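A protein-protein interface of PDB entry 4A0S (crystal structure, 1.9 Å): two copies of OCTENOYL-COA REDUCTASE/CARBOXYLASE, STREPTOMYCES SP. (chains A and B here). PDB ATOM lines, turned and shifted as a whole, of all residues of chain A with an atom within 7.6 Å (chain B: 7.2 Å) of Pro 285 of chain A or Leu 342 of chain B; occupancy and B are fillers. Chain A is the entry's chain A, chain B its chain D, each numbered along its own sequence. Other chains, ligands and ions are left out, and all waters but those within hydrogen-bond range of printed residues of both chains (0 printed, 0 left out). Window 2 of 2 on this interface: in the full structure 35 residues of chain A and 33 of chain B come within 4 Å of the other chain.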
ATOM      1  N   ASP A 280     -24.233 -21.321 -24.085  1.00  0.00           N
ATOM      2  CA  ASP A 280     -24.137 -22.648 -23.527  1.00  0.00           C
ATOM      3  C   ASP A 280     -22.721 -22.897 -23.046  1.00  0.00           C
ATOM      4  O   ASP A 280     -22.441 -23.931 -22.435  1.00  0.00           O
ATOM      5  CB  ASP A 280     -24.537 -23.681 -24.579  1.00  0.00           C
ATOM      6  CG  ASP A 280     -23.709 -23.571 -25.842  1.00  0.00           C
ATOM      7  OD1 ASP A 280     -22.490 -23.797 -25.761  1.00  0.00           O
ATOM      8  OD2 ASP A 280     -24.269 -23.267 -26.915  1.00  0.00           O
ATOM      9  N   ILE A 281     -21.827 -21.944 -23.309  1.00  0.00           N
ATOM     10  CA  ILE A 281     -20.428 -22.111 -22.918  1.00  0.00           C
ATOM     11  C   ILE A 281     -20.285 -22.435 -21.423  1.00  0.00           C
ATOM     12  O   ILE A 281     -19.401 -23.209 -21.031  1.00  0.00           O
ATOM     13  CB  ILE A 281     -19.570 -20.893 -23.310  1.00  0.00           C
ATOM     14  CG1 ILE A 281     -18.086 -21.267 -23.287  1.00  0.00           C
ATOM     15  CG2 ILE A 281     -19.887 -19.677 -22.406  1.00  0.00           C
ATOM     16  CD1 ILE A 281     -17.190 -20.181 -23.814  1.00  0.00           C
ATOM     17  N   ALA A 282     -21.187 -21.875 -20.615  1.00  0.00           N
ATOM     18  CA  ALA A 282     -21.133 -21.974 -19.153  1.00  0.00           C
ATOM     19  C   ALA A 282     -21.254 -23.409 -18.637  1.00  0.00           C
ATOM     20  O   ALA A 282     -20.730 -23.732 -17.569  1.00  0.00           O
ATOM     21  CB  ALA A 282     -22.218 -21.109 -18.543  1.00  0.00           C
ATOM     22  N   ASP A 283     -21.948 -24.249 -19.406  1.00  0.00           N
ATOM     23  CA  ASP A 283     -22.190 -25.661 -19.066  1.00  0.00           C
ATOM     24  C   ASP A 283     -20.984 -26.555 -19.379  1.00  0.00           C
ATOM     25  O   ASP A 283     -20.976 -27.749 -19.060  1.00  0.00           O
ATOM     26  CB  ASP A 283     -23.403 -26.192 -19.845  1.00  0.00           C
ATOM     27  CG  ASP A 283     -24.648 -25.322 -19.685  1.00  0.00           C
ATOM     28  OD1 ASP A 283     -24.820 -24.682 -18.626  1.00  0.00           O
ATOM     29  OD2 ASP A 283     -25.471 -25.298 -20.628  1.00  0.00           O
ATOM     30  N   ASP A 284     -19.969 -25.963 -20.001  1.00  0.00           N
ATOM     31  CA  ASP A 284     -18.868 -26.712 -20.583  1.00  0.00           C
ATOM     32  C   ASP A 284     -17.541 -26.234 -19.986  1.00  0.00           C
ATOM     33  O   ASP A 284     -16.880 -25.366 -20.561  1.00  0.00           O
ATOM     34  CB  ASP A 284     -18.896 -26.512 -22.103  1.00  0.00           C
ATOM     35  CG  ASP A 284     -17.981 -27.466 -22.863  1.00  0.00           C
ATOM     36  OD1 ASP A 284     -16.969 -27.946 -22.312  1.00  0.00           O
ATOM     37  OD2 ASP A 284     -18.269 -27.711 -24.048  1.00  0.00           O
ATOM     38  N   PRO A 285     -17.140 -26.813 -18.836  1.00  0.00           N
ATOM     39  CA  PRO A 285     -15.932 -26.396 -18.118  1.00  0.00           C
ATOM     40  C   PRO A 285     -14.690 -26.330 -19.005  1.00  0.00           C
ATOM     41  O   PRO A 285     -13.922 -25.366 -18.914  1.00  0.00           O
ATOM     42  CB  PRO A 285     -15.764 -27.486 -17.056  1.00  0.00           C
ATOM     43  CG  PRO A 285     -17.128 -27.998 -16.838  1.00  0.00           C
ATOM     44  CD  PRO A 285     -17.790 -27.958 -18.175  1.00  0.00           C
ATOM     45  N   ARG A 286     -14.509 -27.345 -19.852  1.00  0.00           N
ATOM     46  CA  ARG A 286     -13.368 -27.413 -20.754  1.00  0.00           C
ATOM     47  C   ARG A 286     -13.312 -26.225 -21.702  1.00  0.00           C
ATOM     48  O   ARG A 286     -12.275 -25.564 -21.824  1.00  0.00           O
ATOM     49  CB  ARG A 286     -13.385 -28.714 -21.564  1.00  0.00           C
ATOM     50  CG  ARG A 286     -12.170 -28.869 -22.478  1.00  0.00           C
ATOM     51  CD  ARG A 286     -10.908 -28.424 -21.742  1.00  0.00           C
ATOM     52  NE  ARG A 286      -9.674 -28.797 -22.422  1.00  0.00           N
ATOM     53  CZ  ARG A 286      -8.465 -28.676 -21.879  1.00  0.00           C
ATOM     54  NH1 ARG A 286      -8.333 -28.197 -20.645  1.00  0.00           N
ATOM     55  NH2 ARG A 286      -7.386 -29.038 -22.565  1.00  0.00           N
ATOM     56  N   ARG A 287     -14.431 -25.978 -22.378  1.00  0.00           N
ATOM     57  CA  ARG A 287     -14.550 -24.909 -23.309  1.00  0.00           C
ATOM     58  C   ARG A 287     -14.410 -23.564 -22.609  1.00  0.00           C
ATOM     59  O   ARG A 287     -13.769 -22.673 -23.157  1.00  0.00           O
ATOM     60  CB  ARG A 287     -15.896 -24.955 -24.039  1.00  0.00           C
ATOM     61  CG  ARG A 287     -16.061 -23.863 -25.087  1.00  0.00           C
ATOM     62  CD  ARG A 287     -16.897 -24.333 -26.253  1.00  0.00           C
ATOM     63  NE  ARG A 287     -18.327 -24.168 -26.015  1.00  0.00           N
ATOM     64  CZ  ARG A 287     -19.027 -23.085 -26.341  1.00  0.00           C
ATOM     65  NH1 ARG A 287     -18.440 -22.042 -26.916  1.00  0.00           N
ATOM     66  NH2 ARG A 287     -20.323 -23.042 -26.087  1.00  0.00           N
ATOM     67  N   VAL A 288     -14.853 -23.485 -21.347  1.00  0.00           N
ATOM     68  CA  VAL A 288     -14.658 -22.256 -20.578  1.00  0.00           C
ATOM     69  C   VAL A 288     -13.165 -22.037 -20.359  1.00  0.00           C
ATOM     70  O   VAL A 288     -12.676 -20.925 -20.539  1.00  0.00           O
ATOM     71  CB  VAL A 288     -15.458 -22.226 -19.245  1.00  0.00           C
ATOM     72  CG1 VAL A 288     -15.088 -21.006 -18.415  1.00  0.00           C
ATOM     73  CG2 VAL A 288     -16.949 -22.205 -19.524  1.00  0.00           C
ATOM     74  N   VAL A 289     -12.436 -23.101 -20.020  1.00  0.00           N
ATOM     75  CA  VAL A 289     -10.989 -22.980 -19.808  1.00  0.00           C
ATOM     76  C   VAL A 289     -10.281 -22.601 -21.104  1.00  0.00           C
ATOM     77  O   VAL A 289      -9.529 -21.619 -21.137  1.00  0.00           O
ATOM     78  CB  VAL A 289     -10.367 -24.254 -19.174  1.00  0.00           C
ATOM     79  CG1 VAL A 289      -8.847 -24.181 -19.181  1.00  0.00           C
ATOM     80  CG2 VAL A 289     -10.870 -24.429 -17.741  1.00  0.00           C
ATOM     81  N   GLU A 290     -10.536 -23.360 -22.170  1.00  0.00           N
ATOM     82  CA  GLU A 290      -9.942 -23.066 -23.479  1.00  0.00           C
ATOM     83  C   GLU A 290     -10.235 -21.626 -23.880  1.00  0.00           C
ATOM     84  O   GLU A 290      -9.320 -20.864 -24.168  1.00  0.00           O
ATOM     85  CB  GLU A 290     -10.464 -24.004 -24.568  1.00  0.00           C
ATOM     86  CG  GLU A 290     -10.109 -25.462 -24.406  1.00  0.00           C
ATOM     87  CD  GLU A 290     -10.932 -26.349 -25.324  1.00  0.00           C
ATOM     88  OE1 GLU A 290     -12.044 -26.756 -24.923  1.00  0.00           O
ATOM     89  OE2 GLU A 290     -10.485 -26.621 -26.455  1.00  0.00           O
ATOM     90  N   THR A 291     -11.518 -21.270 -23.879  1.00  0.00           N
ATOM     91  CA  THR A 291     -11.966 -19.936 -24.261  1.00  0.00           C
ATOM     92  C   THR A 291     -11.388 -18.864 -23.342  1.00  0.00           C
ATOM     93  O   THR A 291     -10.901 -17.845 -23.822  1.00  0.00           O
ATOM     94  CB  THR A 291     -13.505 -19.843 -24.296  1.00  0.00           C
ATOM     95  OG1 THR A 291     -14.015 -20.822 -25.205  1.00  0.00           O
ATOM     96  CG2 THR A 291     -13.963 -18.455 -24.748  1.00  0.00           C
ATOM     97  N   GLY A 292     -11.425 -19.109 -22.033  1.00  0.00           N
ATOM     98  CA  GLY A 292     -10.808 -18.208 -21.059  1.00  0.00           C
ATOM     99  C   GLY A 292      -9.365 -17.957 -21.432  1.00  0.00           C
ATOM    100  O   GLY A 292      -8.904 -16.813 -21.463  1.00  0.00           O
ATOM    101  N   GLY A 320     -17.368 -17.723 -15.709  1.00  0.00           N
ATOM    102  CA  GLY A 320     -16.314 -18.720 -15.653  1.00  0.00           C
ATOM    103  C   GLY A 320     -15.112 -18.212 -16.403  1.00  0.00           C
ATOM    104  O   GLY A 320     -13.980 -18.395 -15.973  1.00  0.00           O
ATOM    105  N   LEU A 321     -15.368 -17.548 -17.527  1.00  0.00           N
ATOM    106  CA  LEU A 321     -14.307 -16.911 -18.303  1.00  0.00           C
ATOM    107  C   LEU A 321     -13.641 -15.811 -17.479  1.00  0.00           C
ATOM    108  O   LEU A 321     -12.421 -15.742 -17.410  1.00  0.00           O
ATOM    109  CB  LEU A 321     -14.875 -16.330 -19.595  1.00  0.00           C
ATOM    110  CG  LEU A 321     -15.613 -17.345 -20.473  1.00  0.00           C
ATOM    111  CD1 LEU A 321     -16.503 -16.632 -21.490  1.00  0.00           C
ATOM    112  CD2 LEU A 321     -14.589 -18.206 -21.153  1.00  0.00           C
ATOM    113  N   ILE A 324     -11.220 -17.044 -15.106  1.00  0.00           N
ATOM    114  CA  ILE A 324     -10.016 -17.589 -15.727  1.00  0.00           C
ATOM    115  C   ILE A 324      -9.101 -16.483 -16.234  1.00  0.00           C
ATOM    116  O   ILE A 324      -7.883 -16.518 -16.024  1.00  0.00           O
ATOM    117  CB  ILE A 324     -10.370 -18.566 -16.865  1.00  0.00           C
ATOM    118  CG1 ILE A 324     -11.017 -19.821 -16.263  1.00  0.00           C
ATOM    119  CG2 ILE A 324      -9.103 -18.934 -17.668  1.00  0.00           C
ATOM    120  CD1 ILE A 324     -11.777 -20.643 -17.252  1.00  0.00           C
ATOM    121  N   HIS A 343     -23.945 -18.910 -11.367  1.00  0.00           N
ATOM    122  CA  HIS A 343     -22.597 -18.870 -11.899  1.00  0.00           C
ATOM    123  C   HIS A 343     -21.902 -20.160 -11.595  1.00  0.00           C
ATOM    124  O   HIS A 343     -22.055 -20.698 -10.511  1.00  0.00           O
ATOM    125  CB  HIS A 343     -21.826 -17.739 -11.257  1.00  0.00           C
ATOM    126  CG  HIS A 343     -22.259 -16.383 -11.713  1.00  0.00           C
ATOM    127  ND1 HIS A 343     -21.504 -15.254 -11.481  1.00  0.00           N
ATOM    128  CD2 HIS A 343     -23.351 -15.977 -12.408  1.00  0.00           C
ATOM    129  CE1 HIS A 343     -22.120 -14.208 -12.010  1.00  0.00           C
ATOM    130  NE2 HIS A 343     -23.240 -14.621 -12.579  1.00  0.00           N
ATOM    131  N   THR A 344     -21.166 -20.654 -12.580  1.00  0.00           N
ATOM    132  CA  THR A 344     -20.221 -21.732 -12.385  1.00  0.00           C
ATOM    133  C   THR A 344     -18.855 -21.259 -12.816  1.00  0.00           C
ATOM    134  O   THR A 344     -18.706 -20.567 -13.824  1.00  0.00           O
ATOM    135  CB  THR A 344     -20.617 -22.991 -13.162  1.00  0.00           C
ATOM    136  OG1 THR A 344     -21.910 -23.409 -12.718  1.00  0.00           O
ATOM    137  CG2 THR A 344     -19.599 -24.128 -12.937  1.00  0.00           C
ATOM    138  N   PHE A 345     -17.862 -21.610 -12.015  1.00  0.00           N
ATOM    139  CA  PHE A 345     -16.504 -21.254 -12.293  1.00  0.00           C
ATOM    140  C   PHE A 345     -15.607 -22.319 -11.701  1.00  0.00           C
ATOM    141  O   PHE A 345     -16.002 -23.071 -10.802  1.00  0.00           O
ATOM    142  CB  PHE A 345     -16.167 -19.861 -11.733  1.00  0.00           C
ATOM    143  CG  PHE A 345     -16.067 -19.812 -10.236  1.00  0.00           C
ATOM    144  CD1 PHE A 345     -17.208 -19.648  -9.457  1.00  0.00           C
ATOM    145  CD2 PHE A 345     -14.838 -19.956  -9.603  1.00  0.00           C
ATOM    146  CE1 PHE A 345     -17.126 -19.613  -8.054  1.00  0.00           C
ATOM    147  CE2 PHE A 345     -14.743 -19.919  -8.206  1.00  0.00           C
ATOM    148  CZ  PHE A 345     -15.887 -19.752  -7.433  1.00  0.00           C
ATOM    149  N   ASP A 346     -14.393 -22.365 -12.223  1.00  0.00           N
ATOM    150  CA  ASP A 346     -13.386 -23.282 -11.759  1.00  0.00           C
ATOM    151  C   ASP A 346     -12.628 -22.570 -10.638  1.00  0.00           C
ATOM    152  O   ASP A 346     -11.936 -21.577 -10.863  1.00  0.00           O
ATOM    153  CB  ASP A 346     -12.471 -23.644 -12.929  1.00  0.00           C
ATOM    154  CG  ASP A 346     -11.470 -24.728 -12.591  1.00  0.00           C
ATOM    155  OD1 ASP A 346     -11.040 -24.844 -11.426  1.00  0.00           O
ATOM    156  OD2 ASP A 346     -11.099 -25.464 -13.523  1.00  0.00           O
ATOM    157  N   ASN A 347     -12.786 -23.078  -9.428  1.00  0.00           N
ATOM    158  CA  ASN A 347     -12.212 -22.426  -8.261  1.00  0.00           C
ATOM    159  C   ASN A 347     -10.703 -22.512  -8.221  1.00  0.00           C
ATOM    160  O   ASN A 347     -10.057 -21.725  -7.539  1.00  0.00           O
ATOM    161  CB  ASN A 347     -12.795 -22.978  -6.963  1.00  0.00           C
ATOM    162  CG  ASN A 347     -12.462 -22.094  -5.758  1.00  0.00           C
ATOM    163  OD1 ASN A 347     -12.576 -20.863  -5.818  1.00  0.00           O
ATOM    164  ND2 ASN A 347     -12.038 -22.717  -4.672  1.00  0.00           N
ATOM    165  N   ARG A 348     -10.135 -23.452  -8.958  1.00  0.00           N
ATOM    166  CA  ARG A 348      -8.685 -23.532  -9.037  1.00  0.00           C
ATOM    167  C   ARG A 348      -8.101 -22.209  -9.514  1.00  0.00           C
ATOM    168  O   ARG A 348      -7.129 -21.720  -8.957  1.00  0.00           O
ATOM    169  CB  ARG A 348      -8.233 -24.679  -9.930  1.00  0.00           C
ATOM    170  CG  ARG A 348      -8.455 -26.026  -9.279  1.00  0.00           C
ATOM    171  CD  ARG A 348      -8.178 -27.133 -10.256  1.00  0.00           C
ATOM    172  NE  ARG A 348      -8.814 -26.866 -11.546  1.00  0.00           N
ATOM    173  CZ  ARG A 348      -8.497 -27.484 -12.681  1.00  0.00           C
ATOM    174  NH1 ARG A 348      -7.553 -28.415 -12.691  1.00  0.00           N
ATOM    175  NH2 ARG A 348      -9.124 -27.163 -13.808  1.00  0.00           N
ATOM    176  N   TYR A 349      -8.728 -21.613 -10.516  1.00  0.00           N
ATOM    177  CA  TYR A 349      -8.260 -20.328 -11.011  1.00  0.00           C
ATOM    178  C   TYR A 349      -8.422 -19.250  -9.959  1.00  0.00           C
ATOM    179  O   TYR A 349      -7.615 -18.328  -9.881  1.00  0.00           O
ATOM    180  CB  TYR A 349      -8.935 -19.981 -12.338  1.00  0.00           C
ATOM    181  CG  TYR A 349      -8.500 -20.953 -13.400  1.00  0.00           C
ATOM    182  CD1 TYR A 349      -7.320 -20.760 -14.102  1.00  0.00           C
ATOM    183  CD2 TYR A 349      -9.240 -22.115 -13.653  1.00  0.00           C
ATOM    184  CE1 TYR A 349      -6.895 -21.677 -15.061  1.00  0.00           C
ATOM    185  CE2 TYR A 349      -8.830 -23.034 -14.599  1.00  0.00           C
ATOM    186  CZ  TYR A 349      -7.656 -22.810 -15.304  1.00  0.00           C
ATOM    187  OH  TYR A 349      -7.250 -23.719 -16.243  1.00  0.00           O
ATOM    188  N   ALA B 282     -25.089 -28.929  -4.631  1.00  0.00           N
ATOM    189  CA  ALA B 282     -24.629 -27.795  -5.446  1.00  0.00           C
ATOM    190  C   ALA B 282     -25.340 -27.768  -6.790  1.00  0.00           C
ATOM    191  O   ALA B 282     -25.525 -26.703  -7.392  1.00  0.00           O
ATOM    192  CB  ALA B 282     -23.120 -27.868  -5.654  1.00  0.00           C
ATOM    193  N   GLY B 315     -15.200 -26.711  -1.019  1.00  0.00           N
ATOM    194  CA  GLY B 315     -15.401 -26.576  -2.448  1.00  0.00           C
ATOM    195  C   GLY B 315     -16.839 -26.690  -2.894  1.00  0.00           C
ATOM    196  O   GLY B 315     -17.744 -26.285  -2.178  1.00  0.00           O
ATOM    197  N   ARG B 316     -17.036 -27.271  -4.076  1.00  0.00           N
ATOM    198  CA  ARG B 316     -18.302 -27.152  -4.778  1.00  0.00           C
ATOM    199  C   ARG B 316     -19.545 -27.489  -3.953  1.00  0.00           C
ATOM    200  O   ARG B 316     -20.557 -26.828  -4.128  1.00  0.00           O
ATOM    201  CB  ARG B 316     -18.282 -27.920  -6.109  1.00  0.00           C
ATOM    202  CG  ARG B 316     -18.908 -29.292  -6.065  1.00  0.00           C
ATOM    203  CD  ARG B 316     -18.861 -29.960  -7.427  1.00  0.00           C
ATOM    204  NE  ARG B 316     -19.603 -29.186  -8.415  1.00  0.00           N
ATOM    205  CZ  ARG B 316     -20.907 -29.310  -8.645  1.00  0.00           C
ATOM    206  NH1 ARG B 316     -21.636 -30.190  -7.963  1.00  0.00           N
ATOM    207  NH2 ARG B 316     -21.485 -28.546  -9.567  1.00  0.00           N
ATOM    208  N   VAL B 317     -19.482 -28.499  -3.078  1.00  0.00           N
ATOM    209  CA  VAL B 317     -20.679 -28.895  -2.311  1.00  0.00           C
ATOM    210  C   VAL B 317     -21.127 -27.789  -1.366  1.00  0.00           C
ATOM    211  O   VAL B 317     -22.324 -27.585  -1.176  1.00  0.00           O
ATOM    212  CB  VAL B 317     -20.536 -30.218  -1.496  1.00  0.00           C
ATOM    213  CG1 VAL B 317     -20.216 -31.389  -2.391  1.00  0.00           C
ATOM    214  CG2 VAL B 317     -19.512 -30.099  -0.387  1.00  0.00           C
ATOM    215  N   PHE B 319     -19.844 -24.503  -1.484  1.00  0.00           N
ATOM    216  CA  PHE B 319     -19.566 -23.140  -1.921  1.00  0.00           C
ATOM    217  C   PHE B 319     -20.804 -22.277  -2.165  1.00  0.00           C
ATOM    218  O   PHE B 319     -20.820 -21.099  -1.820  1.00  0.00           O
ATOM    219  CB  PHE B 319     -18.639 -23.108  -3.126  1.00  0.00           C
ATOM    220  CG  PHE B 319     -18.127 -21.739  -3.433  1.00  0.00           C
ATOM    221  CD1 PHE B 319     -17.028 -21.233  -2.755  1.00  0.00           C
ATOM    222  CD2 PHE B 319     -18.763 -20.935  -4.373  1.00  0.00           C
ATOM    223  CE1 PHE B 319     -16.539 -19.966  -3.038  1.00  0.00           C
ATOM    224  CE2 PHE B 319     -18.279 -19.659  -4.639  1.00  0.00           C
ATOM    225  CZ  PHE B 319     -17.167 -19.182  -3.964  1.00  0.00           C
ATOM    226  N   SER B 337     -10.833 -26.647  -3.034  1.00  0.00           N
ATOM    227  CA  SER B 337     -12.112 -27.185  -3.458  1.00  0.00           C
ATOM    228  C   SER B 337     -12.131 -28.697  -3.317  1.00  0.00           C
ATOM    229  O   SER B 337     -12.267 -29.387  -4.315  1.00  0.00           O
ATOM    230  CB  SER B 337     -12.360 -26.823  -4.925  1.00  0.00           C
ATOM    231  OG  SER B 337     -12.711 -25.458  -5.063  1.00  0.00           O
ATOM    232  N   SER B 339     -14.251 -31.009  -2.425  1.00  0.00           N
ATOM    233  CA  SER B 339     -15.377 -31.718  -3.041  1.00  0.00           C
ATOM    234  C   SER B 339     -15.552 -31.392  -4.525  1.00  0.00           C
ATOM    235  O   SER B 339     -16.515 -31.840  -5.141  1.00  0.00           O
ATOM    236  CB  SER B 339     -16.670 -31.409  -2.308  1.00  0.00           C
ATOM    237  OG  SER B 339     -17.078 -30.076  -2.561  1.00  0.00           O
ATOM    238  N   GLY B 340     -14.638 -30.610  -5.093  1.00  0.00           N
ATOM    239  CA  GLY B 340     -14.656 -30.364  -6.535  1.00  0.00           C
ATOM    240  C   GLY B 340     -14.552 -28.895  -6.873  1.00  0.00           C
ATOM    241  O   GLY B 340     -15.188 -28.065  -6.242  1.00  0.00           O
ATOM    242  N   TYR B 341     -13.740 -28.572  -7.871  1.00  0.00           N
ATOM    243  CA  TYR B 341     -13.446 -27.168  -8.189  1.00  0.00           C
ATOM    244  C   TYR B 341     -14.487 -26.460  -9.044  1.00  0.00           C
ATOM    245  O   TYR B 341     -14.450 -25.235  -9.179  1.00  0.00           O
ATOM    246  CB  TYR B 341     -12.063 -27.031  -8.819  1.00  0.00           C
ATOM    247  CG  TYR B 341     -11.792 -27.989  -9.953  1.00  0.00           C
ATOM    248  CD1 TYR B 341     -12.382 -27.812 -11.207  1.00  0.00           C
ATOM    249  CD2 TYR B 341     -10.933 -29.071  -9.772  1.00  0.00           C
ATOM    250  CE1 TYR B 341     -12.121 -28.701 -12.250  1.00  0.00           C
ATOM    251  CE2 TYR B 341     -10.663 -29.956 -10.800  1.00  0.00           C
ATOM    252  CZ  TYR B 341     -11.262 -29.772 -12.035  1.00  0.00           C
ATOM    253  OH  TYR B 341     -10.990 -30.666 -13.048  1.00  0.00           O
ATOM    254  N   LEU B 342     -15.405 -27.219  -9.634  1.00  0.00           N
ATOM    255  CA  LEU B 342     -16.490 -26.604 -10.372  1.00  0.00           C
ATOM    256  C   LEU B 342     -17.461 -26.055  -9.366  1.00  0.00           C
ATOM    257  O   LEU B 342     -18.334 -26.766  -8.889  1.00  0.00           O
ATOM    258  CB  LEU B 342     -17.189 -27.600 -11.292  1.00  0.00           C
ATOM    259  CG  LEU B 342     -16.615 -27.830 -12.686  1.00  0.00           C
ATOM    260  CD1 LEU B 342     -17.654 -28.581 -13.510  1.00  0.00           C
ATOM    261  CD2 LEU B 342     -16.248 -26.501 -13.346  1.00  0.00           C
ATOM    262  N   HIS B 343     -17.297 -24.783  -9.032  1.00  0.00           N
ATOM    263  CA  HIS B 343     -18.167 -24.164  -8.059  1.00  0.00           C
ATOM    264  C   HIS B 343     -19.369 -23.567  -8.742  1.00  0.00           C
ATOM    265  O   HIS B 343     -19.255 -22.971  -9.817  1.00  0.00           O
ATOM    266  CB  HIS B 343     -17.436 -23.054  -7.355  1.00  0.00           C
ATOM    267  CG  HIS B 343     -16.482 -23.523  -6.313  1.00  0.00           C
ATOM    268  ND1 HIS B 343     -16.018 -22.689  -5.326  1.00  0.00           N
ATOM    269  CD2 HIS B 343     -15.904 -24.728  -6.090  1.00  0.00           C
ATOM    270  CE1 HIS B 343     -15.201 -23.355  -4.533  1.00  0.00           C
ATOM    271  NE2 HIS B 343     -15.097 -24.588  -4.987  1.00  0.00           N
ATOM    272  N   THR B 344     -20.513 -23.698  -8.093  1.00  0.00           N
ATOM    273  CA  THR B 344     -21.726 -23.080  -8.578  1.00  0.00           C
ATOM    274  C   THR B 344     -22.332 -22.270  -7.459  1.00  0.00           C
ATOM    275  O   THR B 344     -22.456 -22.741  -6.342  1.00  0.00           O
ATOM    276  CB  THR B 344     -22.732 -24.112  -9.110  1.00  0.00           C
ATOM    277  OG1 THR B 344     -22.083 -24.935 -10.090  1.00  0.00           O
ATOM    278  CG2 THR B 344     -23.943 -23.414  -9.749  1.00  0.00           C
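OG1 of Thr 344 of chain A sits at hydrogen-bond distance from OG1 of Thr 344 of chain B (3.0 Å). O of Phe 345 of chain A is in hydrogen-bond range of N of His 343 of chain B (2.8 Å). The side-chain amide nitrogen (ND2) of Asn 347 of chain A is in hydrogen-bond range of the side-chain hydroxyl (OG) of Ser 337 of chain B, 2.8 Å away. O of Tyr 341 of chain B lies within hydrogen-bond range of N of Asn 347 of chain A (2.7 Å). The backbone carbonyl oxygen of Phe 345 of chain A sits close to the backbone carbonyl oxygen of Tyr 341 of chain B (3.1 Å).
The guanidinium group (NH2) of Arg 348 of chain A is in salt-bridge range of the side-chain carboxylate (OD2) of Asp 346 of chain A (2.6 Å). The guanidinium group of Arg 316 of chain B is in hydrogen-bond range of the backbone carbonyl oxygen of Leu 342 of chain B (2.8 Å). The backbone NH (N) of Arg 316 of chain B sits at hydrogen-bond distance from a ring nitrogen (NE2) of His 343 of chain B, 3.4 Å away. A ring nitrogen (NE2) of His 343 of chain B lies within hydrogen-bond range of the side-chain hydroxyl (OG) of Ser 337 of chain B (2.5 Å).
Among the printed residues, pairs that only touch across the chains: Thr 344 of chain A with His 343 of chain B, His 343 of chain A with Thr 344 of chain B, Asn 347 of chain A with His 343 of chain B, Asp 346 of chain A with Tyr 341 of chain B, Arg 348 of chain A with Tyr 341 of chain B, Pro 285 of chain A with Leu 342 of chain B, Phe 345 of chain A with Leu 342 of chain B, Phe 345 of chain A with Phe 319 of chain B and His 343 of chain A with His 343 of chain B.
Of chain B, only Leu 342 comes within 4 Å of Pro 285 of chain A. Leu 342 of chain B touches just these residues of chain A: Pro 285 (3.4 Å) and Phe 345 (3.6 Å). Of the printed residues of chain A, Ser 337 of chain B touches Asn 347. Printed residues of chain B within 4 Å of Phe 345 of chain A: Phe 319 (3.6 Å), Tyr 341 (3.1 Å), Leu 342 (3.6 Å) and His 343 (2.8 Å). Asp 284 of chain A touches none of the printed residues of chain B. The nearest residue of chain B that does not touch Pro 285 of chain A is Tyr 341 of chain B (6.2 Å). The nearest printed residue of chain B that does not touch Asn 347 of chain A is Leu 342 of chain B (4.9 Å).
Hydrophobic or aromatic side chains of chain B that line the printed part of chain A: Phe 319, Tyr 341, Leu 342 and His 343. Among the printed residues, no Asp or Glu carboxylate lies within 4 Å of a Lys or Arg side-chain nitrogen of the other chain.
His 343 of chain A touches its own counterpart, His 343 of chain B. His 343 of chain A touches Thr 344 of chain B, and with the chains exchanged Thr 344 of chain A touches His 343 of chain B. Thr 344 of chain A touches its own counterpart, Thr 344 of chain B. 3 positions are printed for both chains.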
